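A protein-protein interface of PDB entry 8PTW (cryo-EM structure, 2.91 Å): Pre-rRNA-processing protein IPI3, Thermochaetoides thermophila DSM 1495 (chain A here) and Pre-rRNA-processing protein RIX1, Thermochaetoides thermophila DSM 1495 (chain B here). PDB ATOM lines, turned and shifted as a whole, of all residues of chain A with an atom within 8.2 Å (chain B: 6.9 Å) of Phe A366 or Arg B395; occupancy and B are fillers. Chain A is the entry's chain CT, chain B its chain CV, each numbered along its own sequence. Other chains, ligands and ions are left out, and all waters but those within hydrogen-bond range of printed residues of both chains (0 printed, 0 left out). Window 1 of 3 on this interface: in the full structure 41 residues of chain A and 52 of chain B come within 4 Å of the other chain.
N of Phe A361 sits at hydrogen-bond distance from OG1 of Thr B328 (2.8 Å).
O of Thr B328 lies within hydrogen-bond range of NE2 of Gln A360, at 3.5 Å.
The backbone carbonyl oxygen (O) of Asn B325 is in hydrogen-bond range of the guanidinium group (NH2) of Arg B395 (3.3 Å).
N of Glu A362 sits at hydrogen-bond distance from O of Pro A339 (2.8 Å).
The backbone carbonyl oxygen of Leu B396 lies close to the side-chain amide oxygen of Asn B399 (2.9 Å).
The backbone carbonyl oxygen (O) of Phe B324 lies within hydrogen-bond range of the guanidinium group (NH1) of Arg B395 (3.0 Å).
NH1 of Arg B395 is in hydrogen-bond range of O of Asn B326.
The backbone carbonyl oxygen (O) of Gln A360 lies within hydrogen-bond range of the backbone NH (N) of Lys A341 (2.8 Å).
Arg B395 touches Thr A340 (CD to CG2, 3.8 Å).
CE2 of Phe A357 touches CD2 of Leu B396, 3.6 Å away.
CZ of Phe A357 touches OD1 of Asn B399 (3.3 Å).
O of Phe A361 touches CB of Pro B327, at 3.5 Å.
Arg B395 touches Phe A361.
Glu A362 touches Pro B327.
NH2 of Arg B395 touches O of Glu A362, at 3.8 Å.
Pro A363 touches Pro B327 (N to CB, 3.9 Å).
NH1 of Arg B394 touches CB of Phe A366 (3.4 Å).
CD1 of Phe A366 touches NH2 of Arg B395 (3.2 Å).
Of the printed residues of chain B, Phe A357 touches Leu B396 (3.6 Å) and Asn B399 (3.3 Å).
Of the printed residues of chain B, Phe A366 touches Arg B394 (3.4 Å) and Arg B395 (3.2 Å).
Of the printed residues of chain A, Leu B396 touches Phe A357 (3.6 Å).
The nearest printed residue of chain B that does not touch Pro A363 is Arg B395 (5.9 Å).
Printed residues of chain B that touch a printed residue of chain A: Tyr B323, Asn B326, Pro B327, Thr B328, Arg B394, Arg B395, Leu B396, Glu B397 and Asn B399.
Hydrophobic or aromatic side chains of chain B that line the printed part of chain A: Pro B327 and Leu B396.
Hydrophobic or aromatic side chains of chain A that line the printed part of chain B: Pro A339, Phe A357, Phe A361 and Phe A366.
Among the printed residues, 17 pairs touch across the chains.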
ATOM      1  N   LYS A 338     -23.582  22.056  16.968  1.00  0.00           N
ATOM      2  CA  LYS A 338     -23.586  22.519  15.597  1.00  0.00           C
ATOM      3  C   LYS A 338     -22.680  21.625  14.761  1.00  0.00           C
ATOM      4  O   LYS A 338     -21.563  21.314  15.186  1.00  0.00           O
ATOM      5  CB  LYS A 338     -23.127  23.987  15.512  1.00  0.00           C
ATOM      6  CG  LYS A 338     -23.139  24.579  14.114  1.00  0.00           C
ATOM      7  CD  LYS A 338     -22.810  26.066  14.123  1.00  0.00           C
ATOM      8  CE  LYS A 338     -21.347  26.334  14.401  1.00  0.00           C
ATOM      9  NZ  LYS A 338     -21.026  27.782  14.289  1.00  0.00           N
ATOM     10  N   PRO A 339     -23.146  21.167  13.591  1.00  0.00           N
ATOM     11  CA  PRO A 339     -22.377  20.158  12.835  1.00  0.00           C
ATOM     12  C   PRO A 339     -21.025  20.635  12.327  1.00  0.00           C
ATOM     13  O   PRO A 339     -20.171  19.802  12.000  1.00  0.00           O
ATOM     14  CB  PRO A 339     -23.320  19.799  11.676  1.00  0.00           C
ATOM     15  CG  PRO A 339     -24.344  20.883  11.638  1.00  0.00           C
ATOM     16  CD  PRO A 339     -24.491  21.369  13.032  1.00  0.00           C
ATOM     17  N   THR A 340     -20.805  21.940  12.238  1.00  0.00           N
ATOM     18  CA  THR A 340     -19.512  22.489  11.865  1.00  0.00           C
ATOM     19  C   THR A 340     -18.939  23.292  13.025  1.00  0.00           C
ATOM     20  O   THR A 340     -19.648  23.627  13.977  1.00  0.00           O
ATOM     21  CB  THR A 340     -19.622  23.378  10.624  1.00  0.00           C
ATOM     22  OG1 THR A 340     -20.631  24.372  10.834  1.00  0.00           O
ATOM     23  CG2 THR A 340     -19.981  22.548   9.405  1.00  0.00           C
ATOM     24  N   LYS A 341     -17.641  23.571  12.956  1.00  0.00           N
ATOM     25  CA  LYS A 341     -16.983  24.472  13.892  1.00  0.00           C
ATOM     26  C   LYS A 341     -16.133  25.458  13.109  1.00  0.00           C
ATOM     27  O   LYS A 341     -15.388  25.062  12.208  1.00  0.00           O
ATOM     28  CB  LYS A 341     -16.113  23.716  14.899  1.00  0.00           C
ATOM     29  CG  LYS A 341     -15.706  24.568  16.094  1.00  0.00           C
ATOM     30  CD  LYS A 341     -14.301  24.259  16.576  1.00  0.00           C
ATOM     31  CE  LYS A 341     -14.205  22.883  17.202  1.00  0.00           C
ATOM     32  NZ  LYS A 341     -13.176  22.837  18.275  1.00  0.00           N
ATOM     33  N   PHE A 357     -16.607  26.796   0.972  1.00  0.00           N
ATOM     34  CA  PHE A 357     -17.016  26.896   2.366  1.00  0.00           C
ATOM     35  C   PHE A 357     -15.921  26.293   3.234  1.00  0.00           C
ATOM     36  O   PHE A 357     -15.487  25.163   2.988  1.00  0.00           O
ATOM     37  CB  PHE A 357     -18.350  26.176   2.584  1.00  0.00           C
ATOM     38  CG  PHE A 357     -18.807  26.135   4.015  1.00  0.00           C
ATOM     39  CD1 PHE A 357     -19.468  27.215   4.571  1.00  0.00           C
ATOM     40  CD2 PHE A 357     -18.597  25.010   4.795  1.00  0.00           C
ATOM     41  CE1 PHE A 357     -19.901  27.177   5.880  1.00  0.00           C
ATOM     42  CE2 PHE A 357     -19.024  24.970   6.104  1.00  0.00           C
ATOM     43  CZ  PHE A 357     -19.676  26.055   6.647  1.00  0.00           C
ATOM     44  N   ALA A 359     -14.809  25.264   7.018  1.00  0.00           N
ATOM     45  CA  ALA A 359     -15.104  24.975   8.418  1.00  0.00           C
ATOM     46  C   ALA A 359     -14.587  23.579   8.730  1.00  0.00           C
ATOM     47  O   ALA A 359     -14.230  22.814   7.833  1.00  0.00           O
ATOM     48  CB  ALA A 359     -16.597  25.081   8.726  1.00  0.00           C
ATOM     49  N   GLN A 360     -14.548  23.258  10.021  1.00  0.00           N
ATOM     50  CA  GLN A 360     -14.171  21.930  10.488  1.00  0.00           C
ATOM     51  C   GLN A 360     -15.434  21.120  10.745  1.00  0.00           C
ATOM     52  O   GLN A 360     -16.323  21.563  11.479  1.00  0.00           O
ATOM     53  CB  GLN A 360     -13.321  21.999  11.756  1.00  0.00           C
ATOM     54  CG  GLN A 360     -13.024  20.629  12.346  1.00  0.00           C
ATOM     55  CD  GLN A 360     -12.086  20.680  13.529  1.00  0.00           C
ATOM     56  OE1 GLN A 360     -11.584  21.739  13.893  1.00  0.00           O
ATOM     57  NE2 GLN A 360     -11.848  19.528  14.142  1.00  0.00           N
ATOM     58  N   PHE A 361     -15.506  19.937  10.145  1.00  0.00           N
ATOM     59  CA  PHE A 361     -16.672  19.083  10.312  1.00  0.00           C
ATOM     60  C   PHE A 361     -16.609  18.365  11.656  1.00  0.00           C
ATOM     61  O   PHE A 361     -15.590  17.769  12.014  1.00  0.00           O
ATOM     62  CB  PHE A 361     -16.745  18.073   9.167  1.00  0.00           C
ATOM     63  CG  PHE A 361     -17.193  18.660   7.850  1.00  0.00           C
ATOM     64  CD1 PHE A 361     -17.601  19.981   7.754  1.00  0.00           C
ATOM     65  CD2 PHE A 361     -17.199  17.882   6.705  1.00  0.00           C
ATOM     66  CE1 PHE A 361     -18.006  20.511   6.545  1.00  0.00           C
ATOM     67  CE2 PHE A 361     -17.605  18.407   5.495  1.00  0.00           C
ATOM     68  CZ  PHE A 361     -18.008  19.722   5.416  1.00  0.00           C
ATOM     69  N   GLU A 362     -17.713  18.419  12.404  1.00  0.00           N
ATOM     70  CA  GLU A 362     -17.759  17.883  13.756  1.00  0.00           C
ATOM     71  C   GLU A 362     -18.410  16.503  13.784  1.00  0.00           C
ATOM     72  O   GLU A 362     -19.260  16.196  12.944  1.00  0.00           O
ATOM     73  CB  GLU A 362     -18.530  18.824  14.691  1.00  0.00           C
ATOM     74  CG  GLU A 362     -17.806  20.122  14.961  1.00  0.00           C
ATOM     75  CD  GLU A 362     -16.538  19.910  15.756  1.00  0.00           C
ATOM     76  OE1 GLU A 362     -16.564  19.118  16.721  1.00  0.00           O
ATOM     77  OE2 GLU A 362     -15.504  20.510  15.400  1.00  0.00           O
ATOM     78  N   PRO A 363     -18.021  15.644  14.730  1.00  0.00           N
ATOM     79  CA  PRO A 363     -18.681  14.339  14.852  1.00  0.00           C
ATOM     80  C   PRO A 363     -20.108  14.490  15.352  1.00  0.00           C
ATOM     81  O   PRO A 363     -20.352  14.976  16.457  1.00  0.00           O
ATOM     82  CB  PRO A 363     -17.809  13.593  15.868  1.00  0.00           C
ATOM     83  CG  PRO A 363     -16.503  14.305  15.856  1.00  0.00           C
ATOM     84  CD  PRO A 363     -16.832  15.737  15.592  1.00  0.00           C
ATOM     85  N   MET A 364     -21.058  14.063  14.521  1.00  0.00           N
ATOM     86  CA  MET A 364     -22.468  14.219  14.845  1.00  0.00           C
ATOM     87  C   MET A 364     -23.257  12.920  14.795  1.00  0.00           C
ATOM     88  O   MET A 364     -24.486  12.973  14.918  1.00  0.00           O
ATOM     89  CB  MET A 364     -23.122  15.239  13.901  1.00  0.00           C
ATOM     90  CG  MET A 364     -22.521  16.628  13.975  1.00  0.00           C
ATOM     91  SD  MET A 364     -22.644  17.345  15.623  1.00  0.00           S
ATOM     92  CE  MET A 364     -24.421  17.451  15.811  1.00  0.00           C
ATOM     93  N   SER A 365     -22.594  11.769  14.627  1.00  0.00           N
ATOM     94  CA  SER A 365     -23.235  10.450  14.537  1.00  0.00           C
ATOM     95  C   SER A 365     -24.273  10.399  13.416  1.00  0.00           C
ATOM     96  O   SER A 365     -25.363   9.848  13.579  1.00  0.00           O
ATOM     97  CB  SER A 365     -23.855  10.032  15.873  1.00  0.00           C
ATOM     98  OG  SER A 365     -25.158  10.570  16.018  1.00  0.00           O
ATOM     99  N   PHE A 366     -23.933  10.992  12.270  1.00  0.00           N
ATOM    100  CA  PHE A 366     -24.842  10.963  11.129  1.00  0.00           C
ATOM    101  C   PHE A 366     -24.880   9.582  10.490  1.00  0.00           C
ATOM    102  O   PHE A 366     -25.900   9.183   9.916  1.00  0.00           O
ATOM    103  CB  PHE A 366     -24.434  12.021  10.105  1.00  0.00           C
ATOM    104  CG  PHE A 366     -24.811  13.422  10.496  1.00  0.00           C
ATOM    105  CD1 PHE A 366     -24.242  14.508   9.854  1.00  0.00           C
ATOM    106  CD2 PHE A 366     -25.738  13.655  11.500  1.00  0.00           C
ATOM    107  CE1 PHE A 366     -24.583  15.800  10.207  1.00  0.00           C
ATOM    108  CE2 PHE A 366     -26.085  14.946  11.857  1.00  0.00           C
ATOM    109  CZ  PHE A 366     -25.504  16.019  11.209  1.00  0.00           C
ATOM    110  N   THR A 367     -23.781   8.839  10.576  1.00  0.00           N
ATOM    111  CA  THR A 367     -23.712   7.475  10.074  1.00  0.00           C
ATOM    112  C   THR A 367     -23.997   6.505  11.213  1.00  0.00           C
ATOM    113  O   THR A 367     -23.301   6.517  12.233  1.00  0.00           O
ATOM    114  CB  THR A 367     -22.341   7.183   9.462  1.00  0.00           C
ATOM    115  N   LYS A 368     -25.017   5.671  11.036  1.00  0.00           N
ATOM    116  CA  LYS A 368     -25.445   4.719  12.050  1.00  0.00           C
ATOM    117  C   LYS A 368     -25.395   3.308  11.483  1.00  0.00           C
ATOM    118  O   LYS A 368     -25.767   3.079  10.327  1.00  0.00           O
ATOM    119  CB  LYS A 368     -26.860   5.034  12.545  1.00  0.00           C
ATOM    120  N   SER A 369     -24.931   2.367  12.301  1.00  0.00           N
ATOM    121  CA  SER A 369     -24.816   0.972  11.908  1.00  0.00           C
ATOM    122  C   SER A 369     -25.190   0.082  13.084  1.00  0.00           C
ATOM    123  O   SER A 369     -25.281   0.534  14.228  1.00  0.00           O
ATOM    124  CB  SER A 369     -23.399   0.639  11.422  1.00  0.00           C
ATOM    125  N   ASP A 372     -22.322  -0.257  15.582  1.00  0.00           N
ATOM    126  CA  ASP A 372     -22.293   0.770  16.617  1.00  0.00           C
ATOM    127  C   ASP A 372     -23.195   0.394  17.785  1.00  0.00           C
ATOM    128  O   ASP A 372     -22.876   0.679  18.944  1.00  0.00           O
ATOM    129  CB  ASP A 372     -22.704   2.120  16.030  1.00  0.00           C
ATOM    130  CG  ASP A 372     -21.653   2.694  15.100  1.00  0.00           C
ATOM    131  OD1 ASP A 372     -20.453   2.611  15.432  1.00  0.00           O
ATOM    132  OD2 ASP A 372     -22.028   3.226  14.034  1.00  0.00           O
ATOM    133  N   TYR B 323     -18.917  12.274   1.900  1.00  0.00           N
ATOM    134  CA  TYR B 323     -18.005  13.363   2.257  1.00  0.00           C
ATOM    135  C   TYR B 323     -18.632  14.292   3.287  1.00  0.00           C
ATOM    136  O   TYR B 323     -17.969  14.715   4.240  1.00  0.00           O
ATOM    137  CB  TYR B 323     -17.603  14.166   1.021  1.00  0.00           C
ATOM    138  CG  TYR B 323     -16.413  13.613   0.285  1.00  0.00           C
ATOM    139  CD1 TYR B 323     -15.133  13.726   0.807  1.00  0.00           C
ATOM    140  CD2 TYR B 323     -16.569  12.995  -0.942  1.00  0.00           C
ATOM    141  CE1 TYR B 323     -14.047  13.221   0.127  1.00  0.00           C
ATOM    142  CE2 TYR B 323     -15.497  12.490  -1.625  1.00  0.00           C
ATOM    143  CZ  TYR B 323     -14.240  12.603  -1.090  1.00  0.00           C
ATOM    144  OH  TYR B 323     -13.178  12.090  -1.789  1.00  0.00           O
ATOM    145  N   PHE B 324     -19.911  14.622   3.111  1.00  0.00           N
ATOM    146  CA  PHE B 324     -20.579  15.510   4.053  1.00  0.00           C
ATOM    147  C   PHE B 324     -21.045  14.756   5.289  1.00  0.00           C
ATOM    148  O   PHE B 324     -21.349  15.369   6.318  1.00  0.00           O
ATOM    149  CB  PHE B 324     -21.753  16.204   3.367  1.00  0.00           C
ATOM    150  CG  PHE B 324     -21.335  17.225   2.356  1.00  0.00           C
ATOM    151  CD1 PHE B 324     -21.133  18.542   2.726  1.00  0.00           C
ATOM    152  CD2 PHE B 324     -21.121  16.861   1.038  1.00  0.00           C
ATOM    153  CE1 PHE B 324     -20.741  19.478   1.797  1.00  0.00           C
ATOM    154  CE2 PHE B 324     -20.725  17.792   0.106  1.00  0.00           C
ATOM    155  CZ  PHE B 324     -20.536  19.103   0.486  1.00  0.00           C
ATOM    156  N   ASN B 325     -21.119  13.426   5.211  1.00  0.00           N
ATOM    157  CA  ASN B 325     -21.515  12.658   6.392  1.00  0.00           C
ATOM    158  C   ASN B 325     -20.391  12.578   7.425  1.00  0.00           C
ATOM    159  O   ASN B 325     -20.642  12.666   8.632  1.00  0.00           O
ATOM    160  CB  ASN B 325     -21.978  11.261   5.984  1.00  0.00           C
ATOM    161  CG  ASN B 325     -23.396  11.252   5.455  1.00  0.00           C
ATOM    162  OD1 ASN B 325     -24.136  12.222   5.614  1.00  0.00           O
ATOM    163  ND2 ASN B 325     -23.784  10.153   4.820  1.00  0.00           N
ATOM    164  N   ASN B 326     -19.149  12.408   6.976  1.00  0.00           N
ATOM    165  CA  ASN B 326     -18.049  12.140   7.894  1.00  0.00           C
ATOM    166  C   ASN B 326     -17.434  13.437   8.430  1.00  0.00           C
ATOM    167  O   ASN B 326     -17.510  14.483   7.783  1.00  0.00           O
ATOM    168  CB  ASN B 326     -16.978  11.311   7.193  1.00  0.00           C
ATOM    169  CG  ASN B 326     -17.446   9.912   6.881  1.00  0.00           C
ATOM    170  OD1 ASN B 326     -17.544   9.068   7.769  1.00  0.00           O
ATOM    171  ND2 ASN B 326     -17.748   9.657   5.615  1.00  0.00           N
ATOM    172  N   PRO B 327     -16.817  13.393   9.613  1.00  0.00           N
ATOM    173  CA  PRO B 327     -16.145  14.585  10.141  1.00  0.00           C
ATOM    174  C   PRO B 327     -14.737  14.750   9.586  1.00  0.00           C
ATOM    175  O   PRO B 327     -14.205  13.889   8.882  1.00  0.00           O
ATOM    176  CB  PRO B 327     -16.114  14.329  11.648  1.00  0.00           C
ATOM    177  CG  PRO B 327     -16.027  12.857  11.748  1.00  0.00           C
ATOM    178  CD  PRO B 327     -16.885  12.325  10.629  1.00  0.00           C
ATOM    179  N   THR B 328     -14.132  15.890   9.920  1.00  0.00           N
ATOM    180  CA  THR B 328     -12.776  16.234   9.509  1.00  0.00           C
ATOM    181  C   THR B 328     -11.948  16.617  10.728  1.00  0.00           C
ATOM    182  O   THR B 328     -12.485  17.118  11.720  1.00  0.00           O
ATOM    183  CB  THR B 328     -12.764  17.396   8.505  1.00  0.00           C
ATOM    184  OG1 THR B 328     -13.307  18.569   9.121  1.00  0.00           O
ATOM    185  CG2 THR B 328     -13.574  17.060   7.264  1.00  0.00           C
ATOM    186  N   CYS B 390     -29.622  16.778   0.153  1.00  0.00           N
ATOM    187  CA  CYS B 390     -30.075  16.591   1.531  1.00  0.00           C
ATOM    188  C   CYS B 390     -28.905  16.537   2.507  1.00  0.00           C
ATOM    189  O   CYS B 390     -28.956  17.146   3.582  1.00  0.00           O
ATOM    190  CB  CYS B 390     -30.910  15.315   1.643  1.00  0.00           C
ATOM    191  SG  CYS B 390     -32.513  15.379   0.829  1.00  0.00           S
ATOM    192  N   ALA B 391     -27.838  15.817   2.146  1.00  0.00           N
ATOM    193  CA  ALA B 391     -26.670  15.739   3.023  1.00  0.00           C
ATOM    194  C   ALA B 391     -25.953  17.082   3.132  1.00  0.00           C
ATOM    195  O   ALA B 391     -25.475  17.452   4.214  1.00  0.00           O
ATOM    196  CB  ALA B 391     -25.706  14.670   2.527  1.00  0.00           C
ATOM    197  N   ILE B 392     -25.858  17.815   2.016  1.00  0.00           N
ATOM    198  CA  ILE B 392     -25.250  19.145   2.029  1.00  0.00           C
ATOM    199  C   ILE B 392     -26.022  20.074   2.955  1.00  0.00           C
ATOM    200  O   ILE B 392     -25.430  20.803   3.762  1.00  0.00           O
ATOM    201  CB  ILE B 392     -25.168  19.705   0.595  1.00  0.00           C
ATOM    202  CG1 ILE B 392     -24.112  18.959  -0.220  1.00  0.00           C
ATOM    203  CG2 ILE B 392     -24.865  21.185   0.598  1.00  0.00           C
ATOM    204  CD1 ILE B 392     -24.062  19.373  -1.672  1.00  0.00           C
ATOM    205  N   ILE B 393     -27.355  20.038   2.874  1.00  0.00           N
ATOM    206  CA  ILE B 393     -28.192  20.834   3.769  1.00  0.00           C
ATOM    207  C   ILE B 393     -27.984  20.428   5.221  1.00  0.00           C
ATOM    208  O   ILE B 393     -27.820  21.284   6.097  1.00  0.00           O
ATOM    209  CB  ILE B 393     -29.669  20.715   3.358  1.00  0.00           C
ATOM    210  CG1 ILE B 393     -29.910  21.426   2.031  1.00  0.00           C
ATOM    211  CG2 ILE B 393     -30.591  21.228   4.445  1.00  0.00           C
ATOM    212  CD1 ILE B 393     -31.297  21.259   1.536  1.00  0.00           C
ATOM    213  N   ARG B 394     -27.958  19.119   5.494  1.00  0.00           N
ATOM    214  CA  ARG B 394     -27.846  18.638   6.868  1.00  0.00           C
ATOM    215  C   ARG B 394     -26.527  19.059   7.503  1.00  0.00           C
ATOM    216  O   ARG B 394     -26.478  19.400   8.690  1.00  0.00           O
ATOM    217  CB  ARG B 394     -27.994  17.120   6.909  1.00  0.00           C
ATOM    218  CG  ARG B 394     -28.417  16.579   8.262  1.00  0.00           C
ATOM    219  CD  ARG B 394     -27.869  15.185   8.479  1.00  0.00           C
ATOM    220  NE  ARG B 394     -28.054  14.357   7.295  1.00  0.00           N
ATOM    221  CZ  ARG B 394     -27.750  13.068   7.223  1.00  0.00           C
ATOM    222  NH1 ARG B 394     -27.251  12.418   8.260  1.00  0.00           N
ATOM    223  NH2 ARG B 394     -27.953  12.417   6.082  1.00  0.00           N
ATOM    224  N   ARG B 395     -25.440  19.035   6.731  1.00  0.00           N
ATOM    225  CA  ARG B 395     -24.157  19.448   7.291  1.00  0.00           C
ATOM    226  C   ARG B 395     -24.056  20.969   7.405  1.00  0.00           C
ATOM    227  O   ARG B 395     -23.568  21.488   8.415  1.00  0.00           O
ATOM    228  CB  ARG B 395     -23.011  18.865   6.461  1.00  0.00           C
ATOM    229  CG  ARG B 395     -21.591  19.260   6.884  1.00  0.00           C
ATOM    230  CD  ARG B 395     -21.322  19.167   8.391  1.00  0.00           C
ATOM    231  NE  ARG B 395     -21.677  17.893   9.007  1.00  0.00           N
ATOM    232  CZ  ARG B 395     -20.889  16.830   9.044  1.00  0.00           C
ATOM    233  NH1 ARG B 395     -19.722  16.814   8.429  1.00  0.00           N
ATOM    234  NH2 ARG B 395     -21.283  15.753   9.713  1.00  0.00           N
ATOM    235  N   LEU B 396     -24.528  21.712   6.398  1.00  0.00           N
ATOM    236  CA  LEU B 396     -24.259  23.149   6.384  1.00  0.00           C
ATOM    237  C   LEU B 396     -25.213  23.926   7.283  1.00  0.00           C
ATOM    238  O   LEU B 396     -24.836  24.973   7.825  1.00  0.00           O
ATOM    239  CB  LEU B 396     -24.317  23.700   4.960  1.00  0.00           C
ATOM    240  CG  LEU B 396     -23.249  23.246   3.968  1.00  0.00           C
ATOM    241  CD1 LEU B 396     -23.477  23.903   2.620  1.00  0.00           C
ATOM    242  CD2 LEU B 396     -21.864  23.538   4.484  1.00  0.00           C
ATOM    243  N   GLU B 397     -26.453  23.442   7.444  1.00  0.00           N
ATOM    244  CA  GLU B 397     -27.546  24.158   8.099  1.00  0.00           C
ATOM    245  C   GLU B 397     -27.785  25.514   7.443  1.00  0.00           C
ATOM    246  O   GLU B 397     -28.175  25.580   6.274  1.00  0.00           O
ATOM    247  CB  GLU B 397     -27.304  24.316   9.605  1.00  0.00           C
ATOM    248  CG  GLU B 397     -27.378  23.020  10.389  1.00  0.00           C
ATOM    249  CD  GLU B 397     -27.481  23.255  11.883  1.00  0.00           C
ATOM    250  OE1 GLU B 397     -27.057  24.335  12.347  1.00  0.00           O
ATOM    251  OE2 GLU B 397     -27.988  22.363  12.594  1.00  0.00           O
ATOM    252  N   ALA B 398     -27.522  26.601   8.174  1.00  0.00           N
ATOM    253  CA  ALA B 398     -27.883  27.929   7.686  1.00  0.00           C
ATOM    254  C   ALA B 398     -26.936  28.409   6.592  1.00  0.00           C
ATOM    255  O   ALA B 398     -27.216  29.404   5.915  1.00  0.00           O
ATOM    256  CB  ALA B 398     -27.907  28.923   8.846  1.00  0.00           C
ATOM    257  N   ASN B 399     -25.807  27.722   6.403  1.00  0.00           N
ATOM    258  CA  ASN B 399     -24.865  28.129   5.366  1.00  0.00           C
ATOM    259  C   ASN B 399     -25.300  27.657   3.984  1.00  0.00           C
ATOM    260  O   ASN B 399     -24.693  28.042   2.979  1.00  0.00           O
ATOM    261  CB  ASN B 399     -23.467  27.606   5.693  1.00  0.00           C
ATOM    262  CG  ASN B 399     -23.084  27.831   7.141  1.00  0.00           C
ATOM    263  OD1 ASN B 399     -22.663  26.907   7.836  1.00  0.00           O
ATOM    264  ND2 ASN B 399     -23.226  29.066   7.606  1.00  0.00           N
